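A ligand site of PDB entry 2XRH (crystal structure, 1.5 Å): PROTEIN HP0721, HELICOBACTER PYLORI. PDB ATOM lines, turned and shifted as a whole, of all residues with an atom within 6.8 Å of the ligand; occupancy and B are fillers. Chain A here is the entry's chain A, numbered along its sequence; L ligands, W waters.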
ATOM      1  N   MET A  22     -36.669  17.716  26.209  1.00  0.00           N
ATOM      2  CA  MET A  22     -35.366  17.504  26.870  1.00  0.00           C
ATOM      3  C   MET A  22     -34.207  17.693  25.892  1.00  0.00           C
ATOM      4  O   MET A  22     -33.048  17.552  26.276  1.00  0.00           O
ATOM      5  CB  MET A  22     -35.276  16.167  27.579  1.00  0.00           C
ATOM      6  CG  MET A  22     -35.418  15.017  26.725  1.00  0.00           C
ATOM      7  SD  MET A  22     -35.253  13.459  27.658  1.00  0.00           S
ATOM      8  CE  MET A  22     -36.795  13.398  28.514  1.00  0.00           C
ATOM      9  N   ALA A  23     -34.491  18.034  24.630  1.00  0.00           N
ATOM     10  CA  ALA A  23     -33.401  18.233  23.664  1.00  0.00           C
ATOM     11  C   ALA A  23     -32.449  19.300  24.155  1.00  0.00           C
ATOM     12  O   ALA A  23     -32.823  20.378  24.566  1.00  0.00           O
ATOM     13  CB  ALA A  23     -33.930  18.596  22.281  1.00  0.00           C
ATOM     14  N   GLY A  24     -31.185  18.955  24.098  1.00  0.00           N
ATOM     15  CA  GLY A  24     -30.097  19.869  24.533  1.00  0.00           C
ATOM     16  C   GLY A  24     -29.747  19.820  26.011  1.00  0.00           C
ATOM     17  O   GLY A  24     -28.724  20.406  26.417  1.00  0.00           O
ATOM     18  N   VAL A  25     -30.547  19.132  26.809  1.00  0.00           N
ATOM     19  CA  VAL A  25     -30.328  19.036  28.258  1.00  0.00           C
ATOM     20  C   VAL A  25     -30.049  17.633  28.742  1.00  0.00           C
ATOM     21  O   VAL A  25     -29.672  17.469  29.896  1.00  0.00           O
ATOM     22  CB  VAL A  25     -31.501  19.624  29.045  1.00  0.00           C
ATOM     23  CG1 VAL A  25     -31.717  21.028  28.615  1.00  0.00           C
ATOM     24  CG2 VAL A  25     -32.696  18.869  28.845  1.00  0.00           C
ATOM     25  N   VAL A  26     -30.197  16.637  27.867  1.00  0.00           N
ATOM     26  CA  VAL A  26     -29.955  15.249  28.255  1.00  0.00           C
ATOM     27  C   VAL A  26     -28.458  15.123  28.611  1.00  0.00           C
ATOM     28  O   VAL A  26     -27.629  15.681  27.936  1.00  0.00           O
ATOM     29  CB  VAL A  26     -30.330  14.260  27.112  1.00  0.00           C
ATOM     30  CG1 VAL A  26     -29.923  12.837  27.409  1.00  0.00           C
ATOM     31  CG2 VAL A  26     -31.826  14.326  26.798  1.00  0.00           C
ATOM     32  N   ILE A  31     -26.875  10.058  26.401  1.00  0.00           N
ATOM     33  CA  ILE A  31     -27.101  10.551  25.051  1.00  0.00           C
ATOM     34  C   ILE A  31     -27.237   9.446  24.017  1.00  0.00           C
ATOM     35  O   ILE A  31     -28.023   9.605  23.089  1.00  0.00           O
ATOM     36  CB  ILE A  31     -26.101  11.679  24.590  1.00  0.00           C
ATOM     37  CG1 ILE A  31     -26.806  12.672  23.647  1.00  0.00           C
ATOM     38  CG2 ILE A  31     -24.786  11.136  24.025  1.00  0.00           C
ATOM     39  CD1 ILE A  31     -27.912  13.555  24.386  1.00  0.00           C
ATOM     40  N   TYR A  34     -30.719   8.126  24.451  1.00  0.00           N
ATOM     41  CA  TYR A  34     -31.668   9.128  23.956  1.00  0.00           C
ATOM     42  C   TYR A  34     -31.739   9.123  22.444  1.00  0.00           C
ATOM     43  O   TYR A  34     -32.814   9.137  21.859  1.00  0.00           O
ATOM     44  CB  TYR A  34     -31.230  10.489  24.462  1.00  0.00           C
ATOM     45  CG  TYR A  34     -32.101  11.672  24.038  1.00  0.00           C
ATOM     46  CD1 TYR A  34     -33.377  11.846  24.508  1.00  0.00           C
ATOM     47  CD2 TYR A  34     -31.561  12.666  23.230  1.00  0.00           C
ATOM     48  CE1 TYR A  34     -34.144  12.956  24.127  1.00  0.00           C
ATOM     49  CE2 TYR A  34     -32.291  13.764  22.867  1.00  0.00           C
ATOM     50  CZ  TYR A  34     -33.570  13.921  23.299  1.00  0.00           C
ATOM     51  OH  TYR A  34     -34.306  15.034  22.923  1.00  0.00           O
ATOM     52  N   THR A  35     -30.598   9.130  21.798  1.00  0.00           N
ATOM     53  CA  THR A  35     -30.496   9.177  20.349  1.00  0.00           C
ATOM     54  C   THR A  35     -31.091   7.918  19.729  1.00  0.00           C
ATOM     55  O   THR A  35     -31.856   7.997  18.775  1.00  0.00           O
ATOM     56  CB  THR A  35     -29.036   9.327  19.931  1.00  0.00           C
ATOM     57  OG1 THR A  35     -28.492  10.526  20.516  1.00  0.00           O
ATOM     58  CG2 THR A  35     -28.847   9.370  18.434  1.00  0.00           C
ATOM     59  N   LEU A  38     -34.884   8.321  19.947  1.00  0.00           N
ATOM     60  CA  LEU A  38     -35.371   9.278  18.953  1.00  0.00           C
ATOM     61  C   LEU A  38     -35.411   8.646  17.594  1.00  0.00           C
ATOM     62  O   LEU A  38     -36.396   8.788  16.909  1.00  0.00           O
ATOM     63  CB  LEU A  38     -34.473  10.519  18.934  1.00  0.00           C
ATOM     64  CG  LEU A  38     -34.527  11.533  20.065  1.00  0.00           C
ATOM     65  CD1 LEU A  38     -33.528  12.663  19.740  1.00  0.00           C
ATOM     66  CD2 LEU A  38     -35.945  12.072  20.306  1.00  0.00           C
ATOM     67  N   ALA A  61     -33.932  22.331  21.638  1.00  0.00           N
ATOM     68  CA  ALA A  61     -32.495  22.361  21.883  1.00  0.00           C
ATOM     69  C   ALA A  61     -32.064  23.830  21.925  1.00  0.00           C
ATOM     70  O   ALA A  61     -31.266  24.214  22.757  1.00  0.00           O
ATOM     71  CB  ALA A  61     -31.721  21.591  20.810  1.00  0.00           C
ATOM     72  N   PHE A  73     -21.537  25.014  27.134  1.00  0.00           N
ATOM     73  CA  PHE A  73     -22.150  24.330  25.988  1.00  0.00           C
ATOM     74  C   PHE A  73     -21.131  23.477  25.228  1.00  0.00           C
ATOM     75  O   PHE A  73     -21.402  22.316  24.893  1.00  0.00           O
ATOM     76  CB  PHE A  73     -22.803  25.326  25.057  1.00  0.00           C
ATOM     77  CG  PHE A  73     -23.436  24.695  23.869  1.00  0.00           C
ATOM     78  CD1 PHE A  73     -24.632  24.045  23.969  1.00  0.00           C
ATOM     79  CD2 PHE A  73     -22.944  24.920  22.605  1.00  0.00           C
ATOM     80  CE1 PHE A  73     -25.258  23.475  22.854  1.00  0.00           C
ATOM     81  CE2 PHE A  73     -23.585  24.359  21.491  1.00  0.00           C
ATOM     82  CZ  PHE A  73     -24.722  23.642  21.630  1.00  0.00           C
ATOM     83  N   ARG A  76     -20.289  20.314  27.121  1.00  0.00           N
ATOM     84  CA  ARG A  76     -21.312  19.287  26.882  1.00  0.00           C
ATOM     85  C   ARG A  76     -21.224  18.683  25.478  1.00  0.00           C
ATOM     86  O   ARG A  76     -21.314  17.440  25.337  1.00  0.00           O
ATOM     87  CB  ARG A  76     -22.703  19.865  27.141  1.00  0.00           C
ATOM     88  CG  ARG A  76     -23.744  18.826  27.030  1.00  0.00           C
ATOM     89  CD  ARG A  76     -25.127  19.364  27.069  1.00  0.00           C
ATOM     90  NE  ARG A  76     -26.139  18.337  26.808  1.00  0.00           N
ATOM     91  CZ  ARG A  76     -26.676  18.034  25.633  1.00  0.00           C
ATOM     92  NH1 ARG A  76     -26.376  18.634  24.481  1.00  0.00           N
ATOM     93  NH2 ARG A  76     -27.623  17.135  25.602  1.00  0.00           N
ATOM     94  N   GLN A  77     -21.059  19.515  24.465  1.00  0.00           N
ATOM     95  CA  GLN A  77     -21.097  19.040  23.099  1.00  0.00           C
ATOM     96  C   GLN A  77     -19.928  18.123  22.824  1.00  0.00           C
ATOM     97  O   GLN A  77     -20.053  17.121  22.097  1.00  0.00           O
ATOM     98  CB  GLN A  77     -21.169  20.200  22.092  1.00  0.00           C
ATOM     99  CG  GLN A  77     -22.472  20.975  22.004  1.00  0.00           C
ATOM    100  CD  GLN A  77     -23.686  20.074  21.898  1.00  0.00           C
ATOM    101  OE1 GLN A  77     -24.337  19.878  22.873  1.00  0.00           O
ATOM    102  NE2 GLN A  77     -23.941  19.521  20.725  1.00  0.00           N
ATOM    103  N   VAL A  80     -20.771  14.853  24.393  1.00  0.00           N
ATOM    104  CA  VAL A  80     -21.792  14.214  23.601  1.00  0.00           C
ATOM    105  C   VAL A  80     -21.112  13.552  22.391  1.00  0.00           C
ATOM    106  O   VAL A  80     -21.387  12.400  22.085  1.00  0.00           O
ATOM    107  CB  VAL A  80     -22.923  15.187  23.175  1.00  0.00           C
ATOM    108  CG1 VAL A  80     -23.699  14.618  22.016  1.00  0.00           C
ATOM    109  CG2 VAL A  80     -23.855  15.481  24.381  1.00  0.00           C
ATOM    110  N   LEU A  84     -21.205   9.570  21.682  1.00  0.00           N
ATOM    111  CA  LEU A  84     -21.787   9.027  20.496  1.00  0.00           C
ATOM    112  C   LEU A  84     -20.771   8.128  19.781  1.00  0.00           C
ATOM    113  O   LEU A  84     -21.155   7.066  19.271  1.00  0.00           O
ATOM    114  CB  LEU A  84     -22.232  10.125  19.541  1.00  0.00           C
ATOM    115  CG  LEU A  84     -23.518  10.816  19.976  1.00  0.00           C
ATOM    116  CD1 LEU A  84     -23.718  12.134  19.111  1.00  0.00           C
ATOM    117  CD2 LEU A  84     -24.708   9.909  19.919  1.00  0.00           C
ATOM    118  N   MET A  92     -22.484  13.570  14.902  1.00  0.00           N
ATOM    119  CA  MET A  92     -23.319  14.738  14.711  1.00  0.00           C
ATOM    120  C   MET A  92     -22.993  15.386  13.371  1.00  0.00           C
ATOM    121  O   MET A  92     -21.813  15.510  13.005  1.00  0.00           O
ATOM    122  CB  MET A  92     -23.055  15.792  15.804  1.00  0.00           C
ATOM    123  CG  MET A  92     -23.667  15.489  17.162  1.00  0.00           C
ATOM    124  SD  MET A  92     -23.299  16.822  18.353  1.00  0.00           S
ATOM    125  CE  MET A  92     -21.577  16.398  18.579  1.00  0.00           C
ATOM    126  N   ASP A  94     -23.690  18.536  12.850  1.00  0.00           N
ATOM    127  CA  ASP A  94     -23.259  19.862  13.265  1.00  0.00           C
ATOM    128  C   ASP A  94     -22.768  19.783  14.704  1.00  0.00           C
ATOM    129  O   ASP A  94     -23.392  19.112  15.540  1.00  0.00           O
ATOM    130  CB  ASP A  94     -24.464  20.796  13.144  1.00  0.00           C
ATOM    131  CG  ASP A  94     -25.755  20.043  12.741  1.00  0.00           C
ATOM    132  OD1 ASP A  94     -25.933  18.900  13.255  1.00  0.00           O
ATOM    133  OD2 ASP A  94     -26.556  20.541  11.912  1.00  0.00           O
ATOM    134  N   ASP A  95     -21.668  20.451  15.025  1.00  0.00           N
ATOM    135  CA  ASP A  95     -21.165  20.452  16.374  1.00  0.00           C
ATOM    136  C   ASP A  95     -22.085  21.102  17.401  1.00  0.00           C
ATOM    137  O   ASP A  95     -22.077  20.618  18.584  1.00  0.00           O
ATOM    138  CB  ASP A  95     -19.845  21.166  16.462  1.00  0.00           C
ATOM    139  CG  ASP A  95     -18.652  20.301  16.022  1.00  0.00           C
ATOM    140  OD1 ASP A  95     -18.721  19.032  15.855  1.00  0.00           O
ATOM    141  OD2 ASP A  95     -17.587  20.957  15.893  1.00  0.00           O
ATOM    142  N   PHE A  96     -22.823  22.167  16.983  1.00  0.00           N
ATOM    143  CA  PHE A  96     -23.888  22.780  17.833  1.00  0.00           C
ATOM    144  C   PHE A  96     -25.014  21.784  18.118  1.00  0.00           C
ATOM    145  O   PHE A  96     -26.033  22.147  18.716  1.00  0.00           O
ATOM    146  CB  PHE A  96     -24.514  24.082  17.222  1.00  0.00           C
ATOM    147  CG  PHE A  96     -23.677  25.367  17.355  1.00  0.00           C
ATOM    148  CD1 PHE A  96     -23.888  26.290  18.380  1.00  0.00           C
ATOM    149  CD2 PHE A  96     -22.790  25.755  16.339  1.00  0.00           C
ATOM    150  CE1 PHE A  96     -23.100  27.453  18.485  1.00  0.00           C
ATOM    151  CE2 PHE A  96     -22.035  26.948  16.414  1.00  0.00           C
ATOM    152  CZ  PHE A  96     -22.198  27.804  17.498  1.00  0.00           C
ATOM    153  N   GLY A  97     -24.877  20.544  17.652  1.00  0.00           N
ATOM    154  CA  GLY A  97     -25.852  19.497  17.851  1.00  0.00           C
ATOM    155  C   GLY A  97     -27.249  19.779  17.341  1.00  0.00           C
ATOM    156  O   GLY A  97     -27.452  20.239  16.207  1.00  0.00           O
ATOM    157  N   LEU A  98     -28.245  19.533  18.203  1.00  0.00           N
ATOM    158  CA  LEU A  98     -29.605  19.610  17.820  1.00  0.00           C
ATOM    159  C   LEU A  98     -30.072  21.047  17.670  1.00  0.00           C
ATOM    160  O   LEU A  98     -31.136  21.250  17.133  1.00  0.00           O
ATOM    161  CB  LEU A  98     -30.525  18.868  18.809  1.00  0.00           C
ATOM    162  CG  LEU A  98     -30.681  17.358  18.634  1.00  0.00           C
ATOM    163  CD1 LEU A  98     -31.394  16.739  19.846  1.00  0.00           C
ATOM    164  CD2 LEU A  98     -31.346  17.001  17.286  1.00  0.00           C
ATOM    165  N   ARG A  99     -29.311  22.052  18.126  1.00  0.00           N
ATOM    166  CA  ARG A  99     -29.780  23.440  17.948  1.00  0.00           C
ATOM    167  C   ARG A  99     -30.022  23.731  16.521  1.00  0.00           C
ATOM    168  O   ARG A  99     -31.009  24.386  16.229  1.00  0.00           O
ATOM    169  CB  ARG A  99     -28.789  24.513  18.445  1.00  0.00           C
ATOM    170  CG  ARG A  99     -28.427  24.467  19.787  1.00  0.00           C
ATOM    171  CD  ARG A  99     -27.398  25.559  20.120  1.00  0.00           C
ATOM    172  NE  ARG A  99     -27.749  26.899  19.609  1.00  0.00           N
ATOM    173  CZ  ARG A  99     -28.479  27.811  20.235  1.00  0.00           C
ATOM    174  NH1 ARG A  99     -28.958  27.609  21.437  1.00  0.00           N
ATOM    175  NH2 ARG A  99     -28.718  28.977  19.651  1.00  0.00           N
HETATM  176  N1  LIG L   1     -28.505  13.679  20.171  1.00  0.00           N
HETATM  177  C1  LIG L   1     -28.497  14.704  21.050  1.00  0.00           C
HETATM  178  C2  LIG L   1     -27.666  15.819  20.838  1.00  0.00           C
HETATM  179  C3  LIG L   1     -26.827  15.868  19.756  1.00  0.00           C
HETATM  180  C4  LIG L   1     -26.868  14.791  18.878  1.00  0.00           C
HETATM  181  C5  LIG L   1     -27.714  13.714  19.110  1.00  0.00           C
HETATM  182  C6  LIG L   1     -27.583  16.898  21.850  1.00  0.00           C
HETATM  183  O1  LIG L   1     -26.469  17.506  21.955  1.00  0.00           O
HETATM  184  O2  LIG L   1     -28.548  17.121  22.598  1.00  0.00           O
HETATM  185  O   HOH W   1     -27.603  20.457  21.211  1.00  0.00           O
HETATM  186  O   HOH W   2     -30.271  16.198  24.085  1.00  0.00           O
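O1 of the ligand is in salt-bridge range of NH1 of Arg 76 (2.8 Å).
A nitrogen (N1) of the ligand lies within hydrogen-bond range of the side-chain hydroxyl (OG1) of Thr 35.
An oxygen (O1) of the ligand sits close to the side-chain amide oxygen of Gln 77 (3.3 Å).
The guanidinium group of Arg 76 is in hydrogen-bond range of the side-chain amide oxygen of Gln 77 (2.9 Å).
The guanidinium group (NE) of Arg 76 sits close to the backbone carbonyl oxygen (O) of Gly 24.
The guanidinium group (NH2) of Arg 76 sits at hydrogen-bond distance from the backbone carbonyl oxygen (O) of Val 26.
The side-chain hydroxyl of Thr 35 lies within hydrogen-bond range of the backbone carbonyl oxygen of Ile 31 (2.8 Å).
The side-chain amide nitrogen (NE2) of Gln 77 lies within hydrogen-bond range of the side-chain sulfur (SD) of Met 92 (3.7 Å).
The side-chain amide nitrogen of Gln 77 lies close to the backbone NH of Gly 97 (3.4 Å).
The backbone carbonyl oxygen of Asp 95 lies within hydrogen-bond range of the side-chain amide nitrogen of Gln 77 (3.0 Å).
Residues that only touch the ligand: Gly 24 (3.5 Å), Ile 31 (3.6 Å), Met 92 (3.7 Å) and Leu 98 (3.7 Å).
Hydrophobic or aromatic side chains that line the ligand: Ile 31, Met 92 and Leu 98.
Water W2 lies within hydrogen-bond range of O2 of the ligand (2.5 Å), N of Gly 24 (2.9 Å) and NH2 of Arg 76 (3.2 Å).
Water W1 lies within hydrogen-bond range of N of Leu 98, O1 of the ligand and O of Phe 96.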
